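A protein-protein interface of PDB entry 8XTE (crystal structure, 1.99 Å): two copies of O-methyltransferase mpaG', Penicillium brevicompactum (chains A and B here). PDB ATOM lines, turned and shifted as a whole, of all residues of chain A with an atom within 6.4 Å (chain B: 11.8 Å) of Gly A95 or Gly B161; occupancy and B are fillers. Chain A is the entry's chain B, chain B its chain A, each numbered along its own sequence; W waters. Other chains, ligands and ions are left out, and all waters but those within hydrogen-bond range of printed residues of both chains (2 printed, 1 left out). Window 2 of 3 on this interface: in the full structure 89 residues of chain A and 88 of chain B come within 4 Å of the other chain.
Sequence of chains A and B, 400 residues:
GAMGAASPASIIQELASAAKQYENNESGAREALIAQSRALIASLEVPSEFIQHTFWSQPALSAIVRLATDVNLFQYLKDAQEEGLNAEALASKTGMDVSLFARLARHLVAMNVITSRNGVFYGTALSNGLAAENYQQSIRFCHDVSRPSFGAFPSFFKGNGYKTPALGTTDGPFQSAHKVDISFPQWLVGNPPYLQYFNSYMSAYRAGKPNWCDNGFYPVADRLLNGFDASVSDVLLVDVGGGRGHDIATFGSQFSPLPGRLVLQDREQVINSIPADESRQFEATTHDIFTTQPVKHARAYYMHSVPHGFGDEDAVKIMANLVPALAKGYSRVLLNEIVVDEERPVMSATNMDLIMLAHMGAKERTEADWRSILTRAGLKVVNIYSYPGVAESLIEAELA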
ATOM      1  N   VAL A  71      -9.461 -25.900   8.262  1.00  0.00           N
ATOM      2  CA  VAL A  71      -9.726 -24.935   9.321  1.00  0.00           C
ATOM      3  C   VAL A  71      -9.641 -25.550  10.716  1.00  0.00           C
ATOM      4  O   VAL A  71     -10.083 -24.925  11.684  1.00  0.00           O
ATOM      5  CB  VAL A  71     -11.092 -24.247   9.123  1.00  0.00           C
ATOM      6  CG1 VAL A  71     -11.101 -23.433   7.835  1.00  0.00           C
ATOM      7  CG2 VAL A  71     -12.213 -25.286   9.132  1.00  0.00           C
ATOM      8  N   LEU A  90     -16.470 -21.504  17.729  1.00  0.00           N
ATOM      9  CA  LEU A  90     -15.828 -22.234  16.636  1.00  0.00           C
ATOM     10  C   LEU A  90     -15.624 -21.359  15.408  1.00  0.00           C
ATOM     11  O   LEU A  90     -14.629 -21.514  14.693  1.00  0.00           O
ATOM     12  CB  LEU A  90     -16.646 -23.471  16.271  1.00  0.00           C
ATOM     13  CG  LEU A  90     -16.252 -24.750  17.001  1.00  0.00           C
ATOM     14  CD1 LEU A  90     -17.351 -25.786  16.901  1.00  0.00           C
ATOM     15  CD2 LEU A  90     -14.943 -25.280  16.421  1.00  0.00           C
ATOM     16  N   ALA A  91     -16.561 -20.447  15.133  1.00  0.00           N
ATOM     17  CA  ALA A  91     -16.360 -19.514  14.029  1.00  0.00           C
ATOM     18  C   ALA A  91     -15.176 -18.598  14.303  1.00  0.00           C
ATOM     19  O   ALA A  91     -14.428 -18.240  13.386  1.00  0.00           O
ATOM     20  CB  ALA A  91     -17.629 -18.696  13.784  1.00  0.00           C
ATOM     21  N   SER A  92     -14.980 -18.225  15.568  1.00  0.00           N
ATOM     22  CA  SER A  92     -13.860 -17.363  15.919  1.00  0.00           C
ATOM     23  C   SER A  92     -12.532 -18.100  15.770  1.00  0.00           C
ATOM     24  O   SER A  92     -11.557 -17.535  15.260  1.00  0.00           O
ATOM     25  CB  SER A  92     -14.047 -16.834  17.343  1.00  0.00           C
ATOM     26  OG  SER A  92     -13.064 -15.872  17.682  1.00  0.00           O
ATOM     27  N   LYS A  93     -12.476 -19.367  16.192  1.00  0.00           N
ATOM     28  CA  LYS A  93     -11.237 -20.130  16.060  1.00  0.00           C
ATOM     29  C   LYS A  93     -10.935 -20.464  14.604  1.00  0.00           C
ATOM     30  O   LYS A  93      -9.783 -20.370  14.165  1.00  0.00           O
ATOM     31  CB  LYS A  93     -11.307 -21.413  16.888  1.00  0.00           C
ATOM     32  CG  LYS A  93     -11.517 -21.215  18.385  1.00  0.00           C
ATOM     33  CD  LYS A  93     -11.904 -22.537  19.041  1.00  0.00           C
ATOM     34  CE  LYS A  93     -11.630 -22.535  20.536  1.00  0.00           C
ATOM     35  NZ  LYS A  93     -10.378 -21.801  20.884  1.00  0.00           N
ATOM     36  N   THR A  94     -11.951 -20.870  13.843  1.00  0.00           N
ATOM     37  CA  THR A  94     -11.748 -21.295  12.463  1.00  0.00           C
ATOM     38  C   THR A  94     -11.603 -20.134  11.484  1.00  0.00           C
ATOM     39  O   THR A  94     -11.217 -20.366  10.332  1.00  0.00           O
ATOM     40  CB  THR A  94     -12.905 -22.202  12.017  1.00  0.00           C
ATOM     41  OG1 THR A  94     -14.155 -21.505  12.142  1.00  0.00           O
ATOM     42  CG2 THR A  94     -12.947 -23.484  12.846  1.00  0.00           C
ATOM     43  N   GLY A  95     -11.885 -18.903  11.907  1.00  0.00           N
ATOM     44  CA  GLY A  95     -11.861 -17.777  10.993  1.00  0.00           C
ATOM     45  C   GLY A  95     -12.996 -17.772   9.992  1.00  0.00           C
ATOM     46  O   GLY A  95     -12.847 -17.220   8.896  1.00  0.00           O
ATOM     47  N   MET A  96     -14.130 -18.370  10.344  1.00  0.00           N
ATOM     48  CA  MET A  96     -15.264 -18.518   9.450  1.00  0.00           C
ATOM     49  C   MET A  96     -16.386 -17.568   9.840  1.00  0.00           C
ATOM     50  O   MET A  96     -16.551 -17.214  11.010  1.00  0.00           O
ATOM     51  CB  MET A  96     -15.792 -19.955   9.471  1.00  0.00           C
ATOM     52  CG  MET A  96     -14.766 -21.005   9.096  1.00  0.00           C
ATOM     53  SD  MET A  96     -15.528 -22.593   8.718  1.00  0.00           S
ATOM     54  CE  MET A  96     -16.593 -22.137   7.344  1.00  0.00           C
ATOM     55  N   ASP A  97     -17.154 -17.156   8.836  1.00  0.00           N
ATOM     56  CA  ASP A  97     -18.407 -16.464   9.084  1.00  0.00           C
ATOM     57  C   ASP A  97     -19.307 -17.353   9.937  1.00  0.00           C
ATOM     58  O   ASP A  97     -19.420 -18.557   9.688  1.00  0.00           O
ATOM     59  CB  ASP A  97     -19.067 -16.121   7.747  1.00  0.00           C
ATOM     60  CG  ASP A  97     -20.154 -15.085   7.872  1.00  0.00           C
ATOM     61  OD1 ASP A  97     -21.043 -15.243   8.737  1.00  0.00           O
ATOM     62  OD2 ASP A  97     -20.112 -14.100   7.101  1.00  0.00           O
ATOM     63  N   LEU A 100     -22.248 -19.068   8.048  1.00  0.00           N
ATOM     64  CA  LEU A 100     -21.673 -20.122   7.223  1.00  0.00           C
ATOM     65  C   LEU A 100     -21.307 -21.334   8.070  1.00  0.00           C
ATOM     66  O   LEU A 100     -21.749 -22.457   7.793  1.00  0.00           O
ATOM     67  CB  LEU A 100     -20.444 -19.597   6.476  1.00  0.00           C
ATOM     68  CG  LEU A 100     -19.794 -20.617   5.533  1.00  0.00           C
ATOM     69  CD1 LEU A 100     -20.805 -21.187   4.544  1.00  0.00           C
ATOM     70  CD2 LEU A 100     -18.594 -20.021   4.806  1.00  0.00           C
ATOM     71  N   ALA B 152     -16.578 -27.959  -5.292  1.00  0.00           N
ATOM     72  CA  ALA B 152     -15.819 -26.717  -5.225  1.00  0.00           C
ATOM     73  C   ALA B 152     -15.956 -25.998  -3.888  1.00  0.00           C
ATOM     74  O   ALA B 152     -15.364 -24.926  -3.725  1.00  0.00           O
ATOM     75  CB  ALA B 152     -16.249 -25.770  -6.354  1.00  0.00           C
ATOM     76  N   PHE B 153     -16.717 -26.550  -2.935  1.00  0.00           N
ATOM     77  CA  PHE B 153     -16.871 -25.896  -1.634  1.00  0.00           C
ATOM     78  C   PHE B 153     -15.538 -25.629  -0.944  1.00  0.00           C
ATOM     79  O   PHE B 153     -15.318 -24.486  -0.503  1.00  0.00           O
ATOM     80  CB  PHE B 153     -17.791 -26.728  -0.729  1.00  0.00           C
ATOM     81  CG  PHE B 153     -19.251 -26.375  -0.825  1.00  0.00           C
ATOM     82  CD1 PHE B 153     -19.828 -26.038  -2.039  1.00  0.00           C
ATOM     83  CD2 PHE B 153     -20.053 -26.409   0.310  1.00  0.00           C
ATOM     84  CE1 PHE B 153     -21.172 -25.733  -2.122  1.00  0.00           C
ATOM     85  CE2 PHE B 153     -21.398 -26.101   0.239  1.00  0.00           C
ATOM     86  CZ  PHE B 153     -21.961 -25.762  -0.979  1.00  0.00           C
ATOM     87  N   PRO B 154     -14.621 -26.602  -0.800  1.00  0.00           N
ATOM     88  CA  PRO B 154     -13.362 -26.300  -0.089  1.00  0.00           C
ATOM     89  C   PRO B 154     -12.566 -25.166  -0.711  1.00  0.00           C
ATOM     90  O   PRO B 154     -12.185 -24.222  -0.006  1.00  0.00           O
ATOM     91  CB  PRO B 154     -12.600 -27.632  -0.151  1.00  0.00           C
ATOM     92  CG  PRO B 154     -13.643 -28.660  -0.308  1.00  0.00           C
ATOM     93  CD  PRO B 154     -14.728 -28.038  -1.123  1.00  0.00           C
ATOM     94  N   SER B 155     -12.305 -25.228  -2.018  1.00  0.00           N
ATOM     95  CA  SER B 155     -11.488 -24.198  -2.652  1.00  0.00           C
ATOM     96  C   SER B 155     -12.210 -22.855  -2.695  1.00  0.00           C
ATOM     97  O   SER B 155     -11.585 -21.806  -2.498  1.00  0.00           O
ATOM     98  CB  SER B 155     -11.085 -24.641  -4.060  1.00  0.00           C
ATOM     99  OG  SER B 155     -12.224 -24.803  -4.882  1.00  0.00           O
ATOM    100  N   PHE B 156     -13.524 -22.859  -2.936  1.00  0.00           N
ATOM    101  CA  PHE B 156     -14.234 -21.590  -3.061  1.00  0.00           C
ATOM    102  C   PHE B 156     -14.230 -20.813  -1.750  1.00  0.00           C
ATOM    103  O   PHE B 156     -13.947 -19.610  -1.729  1.00  0.00           O
ATOM    104  CB  PHE B 156     -15.670 -21.800  -3.534  1.00  0.00           C
ATOM    105  CG  PHE B 156     -16.453 -20.529  -3.563  1.00  0.00           C
ATOM    106  CD1 PHE B 156     -16.234 -19.599  -4.563  1.00  0.00           C
ATOM    107  CD2 PHE B 156     -17.356 -20.229  -2.554  1.00  0.00           C
ATOM    108  CE1 PHE B 156     -16.923 -18.408  -4.578  1.00  0.00           C
ATOM    109  CE2 PHE B 156     -18.049 -19.037  -2.564  1.00  0.00           C
ATOM    110  CZ  PHE B 156     -17.831 -18.125  -3.576  1.00  0.00           C
ATOM    111  N   PHE B 157     -14.558 -21.476  -0.642  1.00  0.00           N
ATOM    112  CA  PHE B 157     -14.642 -20.750   0.618  1.00  0.00           C
ATOM    113  C   PHE B 157     -13.266 -20.460   1.203  1.00  0.00           C
ATOM    114  O   PHE B 157     -13.099 -19.454   1.895  1.00  0.00           O
ATOM    115  CB  PHE B 157     -15.518 -21.518   1.603  1.00  0.00           C
ATOM    116  CG  PHE B 157     -16.977 -21.448   1.264  1.00  0.00           C
ATOM    117  CD1 PHE B 157     -17.648 -20.233   1.301  1.00  0.00           C
ATOM    118  CD2 PHE B 157     -17.669 -22.584   0.875  1.00  0.00           C
ATOM    119  CE1 PHE B 157     -18.991 -20.156   0.975  1.00  0.00           C
ATOM    120  CE2 PHE B 157     -19.012 -22.516   0.546  1.00  0.00           C
ATOM    121  CZ  PHE B 157     -19.674 -21.299   0.596  1.00  0.00           C
ATOM    122  N   LYS B 158     -12.278 -21.319   0.936  1.00  0.00           N
ATOM    123  CA  LYS B 158     -10.887 -20.953   1.185  1.00  0.00           C
ATOM    124  C   LYS B 158     -10.555 -19.626   0.517  1.00  0.00           C
ATOM    125  O   LYS B 158      -9.995 -18.720   1.144  1.00  0.00           O
ATOM    126  CB  LYS B 158      -9.957 -22.062   0.676  1.00  0.00           C
ATOM    127  CG  LYS B 158      -8.481 -21.937   1.079  1.00  0.00           C
ATOM    128  CD  LYS B 158      -8.295 -21.426   2.506  1.00  0.00           C
ATOM    129  CE  LYS B 158      -7.776 -22.524   3.432  1.00  0.00           C
ATOM    130  NZ  LYS B 158      -7.878 -22.151   4.874  1.00  0.00           N
ATOM    131  N   GLY B 159     -10.933 -19.485  -0.754  1.00  0.00           N
ATOM    132  CA  GLY B 159     -10.569 -18.293  -1.501  1.00  0.00           C
ATOM    133  C   GLY B 159     -11.362 -17.059  -1.109  1.00  0.00           C
ATOM    134  O   GLY B 159     -10.805 -15.961  -1.011  1.00  0.00           O
ATOM    135  N   ASN B 160     -12.668 -17.208  -0.882  1.00  0.00           N
ATOM    136  CA  ASN B 160     -13.483 -16.025  -0.626  1.00  0.00           C
ATOM    137  C   ASN B 160     -13.415 -15.553   0.823  1.00  0.00           C
ATOM    138  O   ASN B 160     -14.033 -14.534   1.152  1.00  0.00           O
ATOM    139  CB  ASN B 160     -14.940 -16.275  -1.070  1.00  0.00           C
ATOM    140  CG  ASN B 160     -15.858 -16.745   0.057  1.00  0.00           C
ATOM    141  OD1 ASN B 160     -15.451 -17.458   0.976  1.00  0.00           O
ATOM    142  ND2 ASN B 160     -17.122 -16.351  -0.029  1.00  0.00           N
ATOM    143  N   GLY B 161     -12.670 -16.245   1.683  1.00  0.00           N
ATOM    144  CA  GLY B 161     -12.503 -15.853   3.067  1.00  0.00           C
ATOM    145  C   GLY B 161     -13.389 -16.570   4.059  1.00  0.00           C
ATOM    146  O   GLY B 161     -13.489 -16.119   5.209  1.00  0.00           O
ATOM    147  N   TYR B 162     -14.025 -17.674   3.659  1.00  0.00           N
ATOM    148  CA  TYR B 162     -15.013 -18.377   4.484  1.00  0.00           C
ATOM    149  C   TYR B 162     -16.155 -17.442   4.870  1.00  0.00           C
ATOM    150  O   TYR B 162     -16.562 -17.356   6.030  1.00  0.00           O
ATOM    151  CB  TYR B 162     -14.365 -19.014   5.716  1.00  0.00           C
ATOM    152  CG  TYR B 162     -13.376 -20.080   5.329  1.00  0.00           C
ATOM    153  CD1 TYR B 162     -13.813 -21.322   4.893  1.00  0.00           C
ATOM    154  CD2 TYR B 162     -12.011 -19.833   5.360  1.00  0.00           C
ATOM    155  CE1 TYR B 162     -12.917 -22.302   4.517  1.00  0.00           C
ATOM    156  CE2 TYR B 162     -11.104 -20.808   4.986  1.00  0.00           C
ATOM    157  CZ  TYR B 162     -11.565 -22.040   4.563  1.00  0.00           C
ATOM    158  OH  TYR B 162     -10.673 -23.014   4.186  1.00  0.00           O
ATOM    159  N   LYS B 163     -16.677 -16.739   3.870  1.00  0.00           N
ATOM    160  CA  LYS B 163     -17.750 -15.780   4.060  1.00  0.00           C
ATOM    161  C   LYS B 163     -18.989 -16.240   3.309  1.00  0.00           C
ATOM    162  O   LYS B 163     -18.897 -16.930   2.288  1.00  0.00           O
ATOM    163  CB  LYS B 163     -17.332 -14.379   3.582  1.00  0.00           C
ATOM    164  CG  LYS B 163     -16.312 -13.705   4.494  1.00  0.00           C
ATOM    165  CD  LYS B 163     -15.177 -13.089   3.697  1.00  0.00           C
ATOM    166  CE  LYS B 163     -14.667 -11.805   4.333  1.00  0.00           C
ATOM    167  NZ  LYS B 163     -13.601 -11.175   3.501  1.00  0.00           N
ATOM    168  N   THR B 164     -20.148 -15.875   3.841  1.00  0.00           N
ATOM    169  CA  THR B 164     -21.388 -16.080   3.113  1.00  0.00           C
ATOM    170  C   THR B 164     -21.337 -15.294   1.805  1.00  0.00           C
ATOM    171  O   THR B 164     -20.861 -14.153   1.789  1.00  0.00           O
ATOM    172  CB  THR B 164     -22.583 -15.628   3.955  1.00  0.00           C
ATOM    173  OG1 THR B 164     -22.686 -16.458   5.121  1.00  0.00           O
ATOM    174  CG2 THR B 164     -23.870 -15.709   3.154  1.00  0.00           C
ATOM    175  N   PRO B 165     -21.769 -15.889   0.681  1.00  0.00           N
ATOM    176  CA  PRO B 165     -21.875 -15.117  -0.566  1.00  0.00           C
ATOM    177  C   PRO B 165     -22.667 -13.830  -0.373  1.00  0.00           C
ATOM    178  O   PRO B 165     -23.844 -13.871   0.002  1.00  0.00           O
ATOM    179  CB  PRO B 165     -22.586 -16.093  -1.510  1.00  0.00           C
ATOM    180  CG  PRO B 165     -22.121 -17.435  -1.034  1.00  0.00           C
ATOM    181  CD  PRO B 165     -22.098 -17.311   0.471  1.00  0.00           C
ATOM    182  N   ALA B 166     -22.020 -12.687  -0.622  1.00  0.00           N
ATOM    183  CA  ALA B 166     -22.620 -11.390  -0.311  1.00  0.00           C
ATOM    184  C   ALA B 166     -23.891 -11.157  -1.120  1.00  0.00           C
ATOM    185  O   ALA B 166     -24.972 -10.943  -0.560  1.00  0.00           O
ATOM    186  CB  ALA B 166     -21.608 -10.274  -0.563  1.00  0.00           C
ATOM    187  N   ASP B 171     -21.927 -14.577  -6.715  1.00  0.00           N
ATOM    188  CA  ASP B 171     -20.656 -14.754  -6.023  1.00  0.00           C
ATOM    189  C   ASP B 171     -20.639 -16.025  -5.181  1.00  0.00           C
ATOM    190  O   ASP B 171     -20.357 -15.971  -3.979  1.00  0.00           O
ATOM    191  CB  ASP B 171     -20.367 -13.524  -5.152  1.00  0.00           C
ATOM    192  CG  ASP B 171     -21.550 -13.133  -4.268  1.00  0.00           C
ATOM    193  OD1 ASP B 171     -22.619 -13.775  -4.372  1.00  0.00           O
ATOM    194  OD2 ASP B 171     -21.413 -12.180  -3.467  1.00  0.00           O
ATOM    195  N   GLY B 172     -20.918 -17.173  -5.796  1.00  0.00           N
ATOM    196  CA  GLY B 172     -21.064 -18.408  -5.060  1.00  0.00           C
ATOM    197  C   GLY B 172     -20.267 -19.568  -5.627  1.00  0.00           C
ATOM    198  O   GLY B 172     -19.583 -19.447  -6.649  1.00  0.00           O
ATOM    199  N   PRO B 173     -20.331 -20.724  -4.956  1.00  0.00           N
ATOM    200  CA  PRO B 173     -19.589 -21.891  -5.460  1.00  0.00           C
ATOM    201  C   PRO B 173     -20.104 -22.404  -6.794  1.00  0.00           C
ATOM    202  O   PRO B 173     -19.328 -23.024  -7.534  1.00  0.00           O
ATOM    203  CB  PRO B 173     -19.748 -22.943  -4.353  1.00  0.00           C
ATOM    204  CG  PRO B 173     -20.648 -22.362  -3.322  1.00  0.00           C
ATOM    205  CD  PRO B 173     -20.910 -20.929  -3.616  1.00  0.00           C
ATOM    206  N   SER B 176     -18.128 -20.635  -9.312  1.00  0.00           N
ATOM    207  CA  SER B 176     -16.738 -21.072  -9.274  1.00  0.00           C
ATOM    208  C   SER B 176     -16.577 -22.448  -9.909  1.00  0.00           C
ATOM    209  O   SER B 176     -15.627 -22.678 -10.666  1.00  0.00           O
ATOM    210  CB  SER B 176     -16.233 -21.074  -7.832  1.00  0.00           C
ATOM    211  OG  SER B 176     -14.921 -21.604  -7.744  1.00  0.00           O
HETATM  212  O   HOH W   1     -22.953 -13.930   6.933  1.00  0.00           O
HETATM  213  O   HOH W   2     -14.646 -14.993   7.868  1.00  0.00           O
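The backbone NH of Asp A97 lies within hydrogen-bond range of the backbone carbonyl oxygen of Tyr B162 (2.9 Å).
The side-chain amide oxygen of Asn B160 sits close to the backbone carbonyl oxygen of Phe B157 (3.2 Å).
O of Phe B157 sits at hydrogen-bond distance from N of Tyr B162 (2.7 Å).
The side-chain hydroxyl of Tyr B162 is in hydrogen-bond range of the side-chain amino group of Lys B158 (3.0 Å).
N of Tyr B162 sits at hydrogen-bond distance from OD1 of Asn B160 (3.0 Å).
ND2 of Asn B160 sits at hydrogen-bond distance from O of Lys B163, at 3.0 Å.
The backbone carbonyl oxygen (O) of Ala A91 lies within hydrogen-bond range of the backbone NH (N) of Met A96 (3.1 Å).
Val A71 touches Tyr B162.
Gly A95 touches Gly B161 (O to O, 3.9 Å).
CB of Tyr B162 touches O of Gly A95 (3.95 Å).
CD1 of Tyr B162 touches CE of Met A96 (3.8 Å).
CB of Asp A97 touches CA of Lys B163, at 3.9 Å.
OD2 of Asp A97 touches N of Thr B164, at 3.7 Å.
Leu A100 touches Phe B157.
Tyr B162 touches Leu A100.
Lys B163 touches Leu A100 (N to CD2, 3.9 Å).
Leu A100 touches Thr B164.
Gly A95 touches two residues of chain B.
Of chain A, only Gly A95 (3.9 Å) comes within 4 Å of Gly B161.
No residue of chain B comes within 4 Å of Ala A91.
No residue of chain B comes within 4 Å of Ser A92.
No residue of chain B comes within 4 Å of Thr A94.
Of chain B, only Tyr B162 comes within 4 Å of Met A96.
Printed residues of chain A within 4 Å of Phe B157: Leu A100 (3.6 Å).
Of the printed residues of chain A, Thr B164 touches Asp A97 and Leu A100.
Of the printed residues of chain B, Val A71 touches Tyr B162 (3.6 Å).
The nearest residue of chain B that does not touch Gly A95 is Lys B163 (6.3 Å).
Printed residues of chain A that touch a printed residue of chain B: Val A71, Gly A95, Met A96, Asp A97 and Leu A100.
Hydrophobic or aromatic side chains of chain A that line the printed part of chain B: Val A71, Met A96 and Leu A100.
Along chain A the printed residues that touch a printed residue of chain B span positions 71 to 100.
Among the printed residues, 11 pairs touch across the chains.
No position is printed for both chains.
Of the 11 pairs that touch across the chains among the printed residues, none has its exchanged pair printed and touching as well.
Water W1 bridges OD2 of Asp A97 (2.9 Å) and OG1 of Thr B164 (3.1 Å).
Water W2 lies within hydrogen-bond range of O of Gly A95 (3.0 Å), O of Gly B161 (3.1 Å) and N of Asp A97 (3.5 Å).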
